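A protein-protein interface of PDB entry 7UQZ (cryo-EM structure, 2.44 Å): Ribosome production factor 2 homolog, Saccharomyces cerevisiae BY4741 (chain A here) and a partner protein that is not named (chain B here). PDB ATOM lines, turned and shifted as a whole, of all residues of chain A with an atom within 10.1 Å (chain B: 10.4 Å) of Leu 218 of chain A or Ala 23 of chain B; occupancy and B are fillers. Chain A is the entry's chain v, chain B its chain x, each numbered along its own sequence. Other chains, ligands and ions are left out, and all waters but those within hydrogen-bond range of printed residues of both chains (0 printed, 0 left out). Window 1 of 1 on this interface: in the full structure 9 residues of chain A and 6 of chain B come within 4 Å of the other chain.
Of the printed residues of chain B, Gln 213 of chain A touches Ile 25 (3.4 Å).
Printed residues of chain B within 4 Å of Gly 214 of chain A: Ile 24.
Of chain B, only Ile 25 (3.7 Å) comes within 4 Å of Gly 215 of chain A.
Of the printed residues of chain B, Lys 216 of chain A touches Asp 99.
Leu 218 of chain A touches three residues of chain B.
No residue of chain B comes within 4 Å of Pro 219 of chain A.
Of chain A, only Leu 218 comes within 4 Å of Val 22 of chain B.
Of the printed residues of chain A, Ala 23 of chain B touches Leu 218 (3.8 Å).
Of chain A, only Gly 214 (3.7 Å) and Leu 218 (3.7 Å) come within 4 Å of Ile 24 of chain B.
Of the printed residues of chain A, Ile 25 of chain B touches Gln 213 (3.4 Å) and Gly 215 (3.7 Å).
Of the printed residues of chain A, Asp 99 of chain B touches Lys 216 (3.3 Å) and Arg 217 (3.6 Å).
Asn 100 of chain B touches none of the printed residues of chain A.
The nearest residue of chain B that does not touch Leu 218 of chain A is Ile 25 of chain B (6.3 Å).
The nearest residue of chain A that does not touch Ala 23 of chain B is Gly 214 of chain A (5.0 Å).
The nearest printed residue of chain B that does not touch Gln 213 of chain A is Ile 24 of chain B (4.4 Å).
Of the 15 printed residues of chain B, 5 touch a printed residue of chain A.
Printed residues of chain B that touch a printed residue of chain A: Val 22, Ala 23, Ile 24, Ile 25 and Asp 99.
Along chain B the printed residues that touch a printed residue of chain A span positions 22 to 99.
Printed residues of chain A that touch a printed residue of chain B: Gln 213, Gly 214, Gly 215, Lys 216, Arg 217 and Leu 218.
Hydrophobic or aromatic side chains of chain A that line the printed part of chain B: Leu 218.
Among the printed residues, 8 pairs touch across the chains.
Among the printed residues, Asp or Glu carboxylates within 4 Å of a Lys or Arg side-chain nitrogen of the other chain: Arg 217 of chain A with Asp 99 of chain B.
The side-chain carboxylate (OD2) of Asp 99 of chain B is in salt-bridge range of the guanidinium group (NH1) of Arg 217 of chain A, at 3.6 Å.
The backbone NH of Gln 213 of chain A sits close to the side-chain hydroxyl of Ser 211 of chain A.
OG of Ser 211 of chain A sits at hydrogen-bond distance from O of Leu 218 of chain A, at 3.1 Å.
The backbone NH of Gly 214 of chain A is in hydrogen-bond range of the side-chain hydroxyl of Ser 211 of chain A (3.0 Å).
Among the printed residues, merely in contact across the chains: Gln 213 of chain A with Ile 25 of chain B (3.4 Å), Gly 214 of chain A with Ile 24 of chain B (3.7 Å), Gly 215 of chain A with Ile 25 of chain B (3.7 Å), Lys 216 of chain A with Asp 99 of chain B (3.3 Å), Leu 218 of chain A with Val 22 of chain B (3.7 Å), Leu 218 of chain A with Ala 23 of chain B (3.8 Å) and Leu 218 of chain A with Ile 24 of chain B (3.7 Å).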
ATOM      1  N   LYS A 207      11.824  -8.662   6.771  1.00  0.00           N
ATOM      2  CA  LYS A 207      11.587  -7.754   7.883  1.00  0.00           C
ATOM      3  C   LYS A 207      10.099  -7.451   7.921  1.00  0.00           C
ATOM      4  O   LYS A 207       9.451  -7.411   6.873  1.00  0.00           O
ATOM      5  CB  LYS A 207      12.394  -6.458   7.743  1.00  0.00           C
ATOM      6  CG  LYS A 207      13.860  -6.588   8.114  1.00  0.00           C
ATOM      7  CD  LYS A 207      14.553  -5.238   8.069  1.00  0.00           C
ATOM      8  CE  LYS A 207      16.004  -5.343   8.504  1.00  0.00           C
ATOM      9  NZ  LYS A 207      16.763  -6.302   7.659  1.00  0.00           N
ATOM     10  N   SER A 208       9.561  -7.248   9.118  1.00  0.00           N
ATOM     11  CA  SER A 208       8.139  -6.995   9.299  1.00  0.00           C
ATOM     12  C   SER A 208       7.924  -5.706  10.078  1.00  0.00           C
ATOM     13  O   SER A 208       8.695  -5.379  10.985  1.00  0.00           O
ATOM     14  CB  SER A 208       7.463  -8.165  10.018  1.00  0.00           C
ATOM     15  OG  SER A 208       8.147  -8.489  11.215  1.00  0.00           O
ATOM     16  N   TYR A 209       6.871  -4.976   9.713  1.00  0.00           N
ATOM     17  CA  TYR A 209       6.496  -3.743  10.386  1.00  0.00           C
ATOM     18  C   TYR A 209       4.980  -3.675  10.482  1.00  0.00           C
ATOM     19  O   TYR A 209       4.262  -4.338   9.729  1.00  0.00           O
ATOM     20  CB  TYR A 209       7.022  -2.501   9.652  1.00  0.00           C
ATOM     21  CG  TYR A 209       8.509  -2.507   9.380  1.00  0.00           C
ATOM     22  CD1 TYR A 209       9.407  -1.995  10.308  1.00  0.00           C
ATOM     23  CD2 TYR A 209       9.015  -3.018   8.192  1.00  0.00           C
ATOM     24  CE1 TYR A 209      10.769  -1.996  10.061  1.00  0.00           C
ATOM     25  CE2 TYR A 209      10.371  -3.024   7.938  1.00  0.00           C
ATOM     26  CZ  TYR A 209      11.243  -2.511   8.873  1.00  0.00           C
ATOM     27  OH  TYR A 209      12.595  -2.517   8.619  1.00  0.00           O
ATOM     28  N   LYS A 210       4.498  -2.868  11.424  1.00  0.00           N
ATOM     29  CA  LYS A 210       3.067  -2.629  11.540  1.00  0.00           C
ATOM     30  C   LYS A 210       2.559  -1.900  10.302  1.00  0.00           C
ATOM     31  O   LYS A 210       3.183  -0.949   9.822  1.00  0.00           O
ATOM     32  CB  LYS A 210       2.763  -1.812  12.795  1.00  0.00           C
ATOM     33  CG  LYS A 210       1.327  -1.923  13.279  1.00  0.00           C
ATOM     34  CD  LYS A 210       1.010  -3.341  13.720  1.00  0.00           C
ATOM     35  CE  LYS A 210      -0.378  -3.437  14.328  1.00  0.00           C
ATOM     36  NZ  LYS A 210      -0.520  -2.567  15.529  1.00  0.00           N
ATOM     37  N   SER A 211       1.422  -2.353   9.781  1.00  0.00           N
ATOM     38  CA  SER A 211       0.886  -1.814   8.538  1.00  0.00           C
ATOM     39  C   SER A 211      -0.209  -0.781   8.745  1.00  0.00           C
ATOM     40  O   SER A 211      -0.454   0.026   7.841  1.00  0.00           O
ATOM     41  CB  SER A 211       0.336  -2.944   7.661  1.00  0.00           C
ATOM     42  OG  SER A 211      -0.842  -3.498   8.222  1.00  0.00           O
ATOM     43  N   ASP A 212      -0.904  -0.825   9.888  1.00  0.00           N
ATOM     44  CA  ASP A 212      -1.970   0.110  10.250  1.00  0.00           C
ATOM     45  C   ASP A 212      -3.157   0.025   9.289  1.00  0.00           C
ATOM     46  O   ASP A 212      -4.081   0.842   9.361  1.00  0.00           O
ATOM     47  CB  ASP A 212      -1.426   1.544  10.321  1.00  0.00           C
ATOM     48  CG  ASP A 212      -2.268   2.451  11.197  1.00  0.00           C
ATOM     49  OD1 ASP A 212      -3.217   1.956  11.839  1.00  0.00           O
ATOM     50  OD2 ASP A 212      -1.975   3.665  11.243  1.00  0.00           O
ATOM     51  N   GLN A 213      -3.148  -0.960   8.390  1.00  0.00           N
ATOM     52  CA  GLN A 213      -4.256  -1.197   7.473  1.00  0.00           C
ATOM     53  C   GLN A 213      -4.658  -2.657   7.353  1.00  0.00           C
ATOM     54  O   GLN A 213      -5.810  -2.928   6.995  1.00  0.00           O
ATOM     55  CB  GLN A 213      -3.923  -0.665   6.071  1.00  0.00           C
ATOM     56  CG  GLN A 213      -3.824   0.851   5.985  1.00  0.00           C
ATOM     57  CD  GLN A 213      -3.570   1.339   4.573  1.00  0.00           C
ATOM     58  OE1 GLN A 213      -3.370   0.543   3.655  1.00  0.00           O
ATOM     59  NE2 GLN A 213      -3.578   2.654   4.392  1.00  0.00           N
ATOM     60  N   GLY A 214      -3.763  -3.600   7.635  1.00  0.00           N
ATOM     61  CA  GLY A 214      -4.111  -5.006   7.619  1.00  0.00           C
ATOM     62  C   GLY A 214      -4.318  -5.549   9.015  1.00  0.00           C
ATOM     63  O   GLY A 214      -4.335  -6.765   9.224  1.00  0.00           O
ATOM     64  N   GLY A 215      -4.474  -4.647   9.983  1.00  0.00           N
ATOM     65  CA  GLY A 215      -4.645  -5.038  11.364  1.00  0.00           C
ATOM     66  C   GLY A 215      -3.337  -5.475  12.005  1.00  0.00           C
ATOM     67  O   GLY A 215      -2.243  -5.283  11.474  1.00  0.00           O
ATOM     68  N   LYS A 216      -3.477  -6.082  13.181  1.00  0.00           N
ATOM     69  CA  LYS A 216      -2.340  -6.595  13.933  1.00  0.00           C
ATOM     70  C   LYS A 216      -2.007  -8.036  13.572  1.00  0.00           C
ATOM     71  O   LYS A 216      -1.127  -8.633  14.200  1.00  0.00           O
ATOM     72  CB  LYS A 216      -2.604  -6.480  15.437  1.00  0.00           C
ATOM     73  CG  LYS A 216      -3.778  -7.305  15.930  1.00  0.00           C
ATOM     74  CD  LYS A 216      -4.006  -7.108  17.421  1.00  0.00           C
ATOM     75  CE  LYS A 216      -2.809  -7.575  18.236  1.00  0.00           C
ATOM     76  NZ  LYS A 216      -2.487  -9.006  17.976  1.00  0.00           N
ATOM     77  N   ARG A 217      -2.691  -8.605  12.579  1.00  0.00           N
ATOM     78  CA  ARG A 217      -2.427  -9.961  12.125  1.00  0.00           C
ATOM     79  C   ARG A 217      -1.690 -10.025  10.797  1.00  0.00           C
ATOM     80  O   ARG A 217      -1.149 -11.083  10.463  1.00  0.00           O
ATOM     81  CB  ARG A 217      -3.743 -10.741  11.998  1.00  0.00           C
ATOM     82  CG  ARG A 217      -4.707 -10.510  13.148  1.00  0.00           C
ATOM     83  CD  ARG A 217      -4.212 -11.157  14.426  1.00  0.00           C
ATOM     84  NE  ARG A 217      -4.322 -12.609  14.371  1.00  0.00           N
ATOM     85  CZ  ARG A 217      -5.382 -13.292  14.778  1.00  0.00           C
ATOM     86  NH1 ARG A 217      -6.441 -12.686  15.289  1.00  0.00           N
ATOM     87  NH2 ARG A 217      -5.380 -14.618  14.670  1.00  0.00           N
ATOM     88  N   LEU A 218      -1.658  -8.934  10.034  1.00  0.00           N
ATOM     89  CA  LEU A 218      -1.000  -8.896   8.728  1.00  0.00           C
ATOM     90  C   LEU A 218       0.012  -7.760   8.691  1.00  0.00           C
ATOM     91  O   LEU A 218      -0.364  -6.598   8.451  1.00  0.00           O
ATOM     92  CB  LEU A 218      -2.027  -8.733   7.610  1.00  0.00           C
ATOM     93  CG  LEU A 218      -3.105  -9.814   7.530  1.00  0.00           C
ATOM     94  CD1 LEU A 218      -4.076  -9.516   6.402  1.00  0.00           C
ATOM     95  CD2 LEU A 218      -2.473 -11.186   7.353  1.00  0.00           C
ATOM     96  N   PRO A 219       1.292  -8.030   8.924  1.00  0.00           N
ATOM     97  CA  PRO A 219       2.301  -6.969   8.894  1.00  0.00           C
ATOM     98  C   PRO A 219       2.850  -6.720   7.495  1.00  0.00           C
ATOM     99  O   PRO A 219       2.832  -7.586   6.619  1.00  0.00           O
ATOM    100  CB  PRO A 219       3.398  -7.519   9.815  1.00  0.00           C
ATOM    101  CG  PRO A 219       3.310  -8.992   9.624  1.00  0.00           C
ATOM    102  CD  PRO A 219       1.854  -9.313   9.382  1.00  0.00           C
ATOM    103  N   ARG A 220       3.346  -5.498   7.305  1.00  0.00           N
ATOM    104  CA  ARG A 220       3.988  -5.128   6.051  1.00  0.00           C
ATOM    105  C   ARG A 220       5.357  -5.790   5.948  1.00  0.00           C
ATOM    106  O   ARG A 220       6.158  -5.731   6.885  1.00  0.00           O
ATOM    107  CB  ARG A 220       4.121  -3.608   5.957  1.00  0.00           C
ATOM    108  CG  ARG A 220       5.023  -3.112   4.834  1.00  0.00           C
ATOM    109  CD  ARG A 220       4.336  -3.166   3.479  1.00  0.00           C
ATOM    110  NE  ARG A 220       5.194  -2.635   2.426  1.00  0.00           N
ATOM    111  CZ  ARG A 220       4.815  -2.441   1.171  1.00  0.00           C
ATOM    112  NH1 ARG A 220       3.585  -2.717   0.769  1.00  0.00           N
ATOM    113  NH2 ARG A 220       5.692  -1.958   0.296  1.00  0.00           N
ATOM    114  N   ILE A 221       5.626  -6.411   4.807  1.00  0.00           N
ATOM    115  CA  ILE A 221       6.852  -7.169   4.593  1.00  0.00           C
ATOM    116  C   ILE A 221       7.850  -6.303   3.836  1.00  0.00           C
ATOM    117  O   ILE A 221       7.476  -5.475   2.998  1.00  0.00           O
ATOM    118  CB  ILE A 221       6.557  -8.487   3.841  1.00  0.00           C
ATOM    119  CG1 ILE A 221       5.395  -9.226   4.506  1.00  0.00           C
ATOM    120  CG2 ILE A 221       7.775  -9.393   3.827  1.00  0.00           C
ATOM    121  CD1 ILE A 221       5.677  -9.649   5.931  1.00  0.00           C
ATOM    122  N   ARG B  20      -6.126 -20.279   0.760  1.00  0.00           N
ATOM    123  CA  ARG B  20      -6.830 -19.749   1.916  1.00  0.00           C
ATOM    124  C   ARG B  20      -7.301 -18.321   1.663  1.00  0.00           C
ATOM    125  O   ARG B  20      -6.655 -17.539   0.962  1.00  0.00           O
ATOM    126  CB  ARG B  20      -5.930 -19.787   3.152  1.00  0.00           C
ATOM    127  CG  ARG B  20      -5.474 -21.181   3.544  1.00  0.00           C
ATOM    128  CD  ARG B  20      -6.612 -21.973   4.154  1.00  0.00           C
ATOM    129  NE  ARG B  20      -6.974 -21.467   5.472  1.00  0.00           N
ATOM    130  CZ  ARG B  20      -8.021 -21.879   6.170  1.00  0.00           C
ATOM    131  NH1 ARG B  20      -8.851 -22.795   5.698  1.00  0.00           N
ATOM    132  NH2 ARG B  20      -8.244 -21.359   7.374  1.00  0.00           N
ATOM    133  N   GLU B  21      -8.446 -17.990   2.249  1.00  0.00           N
ATOM    134  CA  GLU B  21      -8.957 -16.629   2.222  1.00  0.00           C
ATOM    135  C   GLU B  21      -8.184 -15.770   3.212  1.00  0.00           C
ATOM    136  O   GLU B  21      -7.671 -16.260   4.221  1.00  0.00           O
ATOM    137  CB  GLU B  21     -10.454 -16.600   2.549  1.00  0.00           C
ATOM    138  CG  GLU B  21     -10.834 -17.265   3.869  1.00  0.00           C
ATOM    139  CD  GLU B  21     -10.772 -16.318   5.053  1.00  0.00           C
ATOM    140  OE1 GLU B  21     -10.753 -15.088   4.834  1.00  0.00           O
ATOM    141  OE2 GLU B  21     -10.741 -16.802   6.204  1.00  0.00           O
ATOM    142  N   VAL B  22      -8.104 -14.477   2.916  1.00  0.00           N
ATOM    143  CA  VAL B  22      -7.379 -13.524   3.747  1.00  0.00           C
ATOM    144  C   VAL B  22      -8.384 -12.536   4.320  1.00  0.00           C
ATOM    145  O   VAL B  22      -9.156 -11.919   3.576  1.00  0.00           O
ATOM    146  CB  VAL B  22      -6.278 -12.804   2.954  1.00  0.00           C
ATOM    147  CG1 VAL B  22      -5.565 -11.801   3.840  1.00  0.00           C
ATOM    148  CG2 VAL B  22      -5.291 -13.813   2.391  1.00  0.00           C
ATOM    149  N   ALA B  23      -8.382 -12.396   5.643  1.00  0.00           N
ATOM    150  CA  ALA B  23      -9.266 -11.457   6.331  1.00  0.00           C
ATOM    151  C   ALA B  23      -8.595 -10.092   6.335  1.00  0.00           C
ATOM    152  O   ALA B  23      -7.787  -9.770   7.208  1.00  0.00           O
ATOM    153  CB  ALA B  23      -9.572 -11.937   7.744  1.00  0.00           C
ATOM    154  N   ILE B  24      -8.940  -9.276   5.345  1.00  0.00           N
ATOM    155  CA  ILE B  24      -8.382  -7.939   5.193  1.00  0.00           C
ATOM    156  C   ILE B  24      -9.474  -6.923   5.503  1.00  0.00           C
ATOM    157  O   ILE B  24     -10.670  -7.191   5.331  1.00  0.00           O
ATOM    158  CB  ILE B  24      -7.789  -7.740   3.778  1.00  0.00           C
ATOM    159  CG1 ILE B  24      -6.871  -6.516   3.734  1.00  0.00           C
ATOM    160  CG2 ILE B  24      -8.887  -7.638   2.726  1.00  0.00           C
ATOM    161  CD1 ILE B  24      -5.692  -6.607   4.674  1.00  0.00           C
ATOM    162  N   ILE B  25      -9.060  -5.763   5.993  1.00  0.00           N
ATOM    163  CA  ILE B  25     -10.009  -4.713   6.374  1.00  0.00           C
ATOM    164  C   ILE B  25     -10.499  -4.007   5.113  1.00  0.00           C
ATOM    165  O   ILE B  25      -9.671  -3.566   4.300  1.00  0.00           O
ATOM    166  CB  ILE B  25      -9.357  -3.726   7.336  1.00  0.00           C
ATOM    167  CG1 ILE B  25      -8.730  -4.468   8.517  1.00  0.00           C
ATOM    168  CG2 ILE B  25     -10.383  -2.723   7.832  1.00  0.00           C
ATOM    169  CD1 ILE B  25      -7.983  -3.567   9.474  1.00  0.00           C
ATOM    170  N   PRO B  26     -11.812  -3.894   4.907  1.00  0.00           N
ATOM    171  CA  PRO B  26     -12.317  -3.176   3.728  1.00  0.00           C
ATOM    172  C   PRO B  26     -12.008  -1.688   3.800  1.00  0.00           C
ATOM    173  O   PRO B  26     -11.927  -1.102   4.882  1.00  0.00           O
ATOM    174  CB  PRO B  26     -13.829  -3.436   3.772  1.00  0.00           C
ATOM    175  CG  PRO B  26     -13.999  -4.617   4.679  1.00  0.00           C
ATOM    176  CD  PRO B  26     -12.896  -4.511   5.685  1.00  0.00           C
ATOM    177  N   LYS B  27     -11.842  -1.076   2.627  1.00  0.00           N
ATOM    178  CA  LYS B  27     -11.522   0.345   2.543  1.00  0.00           C
ATOM    179  C   LYS B  27     -12.754   1.226   2.371  1.00  0.00           C
ATOM    180  O   LYS B  27     -12.720   2.402   2.750  1.00  0.00           O
ATOM    181  CB  LYS B  27     -10.547   0.596   1.388  1.00  0.00           C
ATOM    182  CG  LYS B  27      -9.210  -0.112   1.548  1.00  0.00           C
ATOM    183  CD  LYS B  27      -8.300   0.134   0.360  1.00  0.00           C
ATOM    184  CE  LYS B  27      -7.011  -0.661   0.482  1.00  0.00           C
ATOM    185  NZ  LYS B  27      -6.138  -0.492  -0.712  1.00  0.00           N
ATOM    186  N   ASP B  99      -9.759  -7.150  18.451  1.00  0.00           N
ATOM    187  CA  ASP B  99      -8.838  -6.322  17.682  1.00  0.00           C
ATOM    188  C   ASP B  99      -9.501  -5.085  17.099  1.00  0.00           C
ATOM    189  O   ASP B  99      -9.005  -3.969  17.300  1.00  0.00           O
ATOM    190  CB  ASP B  99      -8.202  -7.148  16.552  1.00  0.00           C
ATOM    191  CG  ASP B  99      -7.455  -8.362  17.065  1.00  0.00           C
ATOM    192  OD1 ASP B  99      -6.981  -8.325  18.219  1.00  0.00           O
ATOM    193  OD2 ASP B  99      -7.343  -9.352  16.312  1.00  0.00           O
ATOM    194  N   ASN B 100     -10.605  -5.249  16.374  1.00  0.00           N
ATOM    195  CA  ASN B 100     -11.291  -4.120  15.765  1.00  0.00           C
ATOM    196  C   ASN B 100     -12.774  -4.439  15.665  1.00  0.00           C
ATOM    197  O   ASN B 100     -13.191  -5.598  15.753  1.00  0.00           O
ATOM    198  CB  ASN B 100     -10.714  -3.778  14.387  1.00  0.00           C
ATOM    199  CG  ASN B 100     -10.908  -4.892  13.379  1.00  0.00           C
ATOM    200  OD1 ASN B 100     -11.955  -4.990  12.737  1.00  0.00           O
ATOM    201  ND2 ASN B 100      -9.896  -5.740  13.231  1.00  0.00           N
ATOM    202  N   TYR B 102     -14.877  -4.204  13.115  1.00  0.00           N
ATOM    203  CA  TYR B 102     -15.302  -4.947  11.931  1.00  0.00           C
ATOM    204  C   TYR B 102     -15.101  -6.445  12.115  1.00  0.00           C
ATOM    205  O   TYR B 102     -16.020  -7.239  11.883  1.00  0.00           O
ATOM    206  CB  TYR B 102     -14.542  -4.459  10.696  1.00  0.00           C
ATOM    207  CG  TYR B 102     -14.750  -5.338   9.482  1.00  0.00           C
ATOM    208  CD1 TYR B 102     -15.916  -5.253   8.735  1.00  0.00           C
ATOM    209  CD2 TYR B 102     -13.785  -6.258   9.086  1.00  0.00           C
ATOM    210  CE1 TYR B 102     -16.119  -6.055   7.630  1.00  0.00           C
ATOM    211  CE2 TYR B 102     -13.980  -7.066   7.983  1.00  0.00           C
ATOM    212  CZ  TYR B 102     -15.148  -6.958   7.258  1.00  0.00           C
ATOM    213  OH  TYR B 102     -15.347  -7.756   6.156  1.00  0.00           O
ATOM    214  N   SER B 103     -13.899  -6.851  12.527  1.00  0.00           N
ATOM    215  CA  SER B 103     -13.627  -8.269  12.721  1.00  0.00           C
ATOM    216  C   SER B 103     -14.368  -8.840  13.920  1.00  0.00           C
ATOM    217  O   SER B 103     -14.748 -10.016  13.894  1.00  0.00           O
ATOM    218  CB  SER B 103     -12.125  -8.503  12.880  1.00  0.00           C
ATOM    219  OG  SER B 103     -11.632  -7.868  14.045  1.00  0.00           O
ATOM    220  N   SER B 104     -14.588  -8.039  14.966  1.00  0.00           N
ATOM    221  CA  SER B 104     -15.251  -8.554  16.156  1.00  0.00           C
ATOM    222  C   SER B 104     -16.745  -8.760  15.933  1.00  0.00           C
ATOM    223  O   SER B 104     -17.299  -9.781  16.356  1.00  0.00           O
ATOM    224  CB  SER B 104     -15.016  -7.612  17.336  1.00  0.00           C
ATOM    225  OG  SER B 104     -13.645  -7.568  17.690  1.00  0.00           O
ATOM    226  N   LYS B 107     -17.710  -8.614  10.778  1.00  0.00           N
ATOM    227  CA  LYS B 107     -17.292  -9.794  10.021  1.00  0.00           C
ATOM    228  C   LYS B 107     -18.115 -11.045  10.336  1.00  0.00           C
ATOM    229  O   LYS B 107     -18.469 -11.762   9.384  1.00  0.00           O
ATOM    230  CB  LYS B 107     -15.792 -10.045  10.225  1.00  0.00           C
ATOM    231  CG  LYS B 107     -15.256 -11.246   9.464  1.00  0.00           C
ATOM    232  CD  LYS B 107     -13.842 -11.588   9.895  1.00  0.00           C
ATOM    233  CE  LYS B 107     -13.357 -12.862   9.227  1.00  0.00           C
ATOM    234  NZ  LYS B 107     -12.003 -13.256   9.702  1.00  0.00           N
ATOM    235  N   PRO B 108     -18.442 -11.379  11.593  1.00  0.00           N
ATOM    236  CA  PRO B 108     -19.430 -12.450  11.811  1.00  0.00           C
ATOM    237  C   PRO B 108     -20.812 -12.126  11.264  1.00  0.00           C
ATOM    238  O   PRO B 108     -21.607 -13.049  11.052  1.00  0.00           O
ATOM    239  CB  PRO B 108     -19.454 -12.604  13.337  1.00  0.00           C
ATOM    240  CG  PRO B 108     -18.131 -12.128  13.778  1.00  0.00           C
ATOM    241  CD  PRO B 108     -17.808 -10.985  12.868  1.00  0.00           C
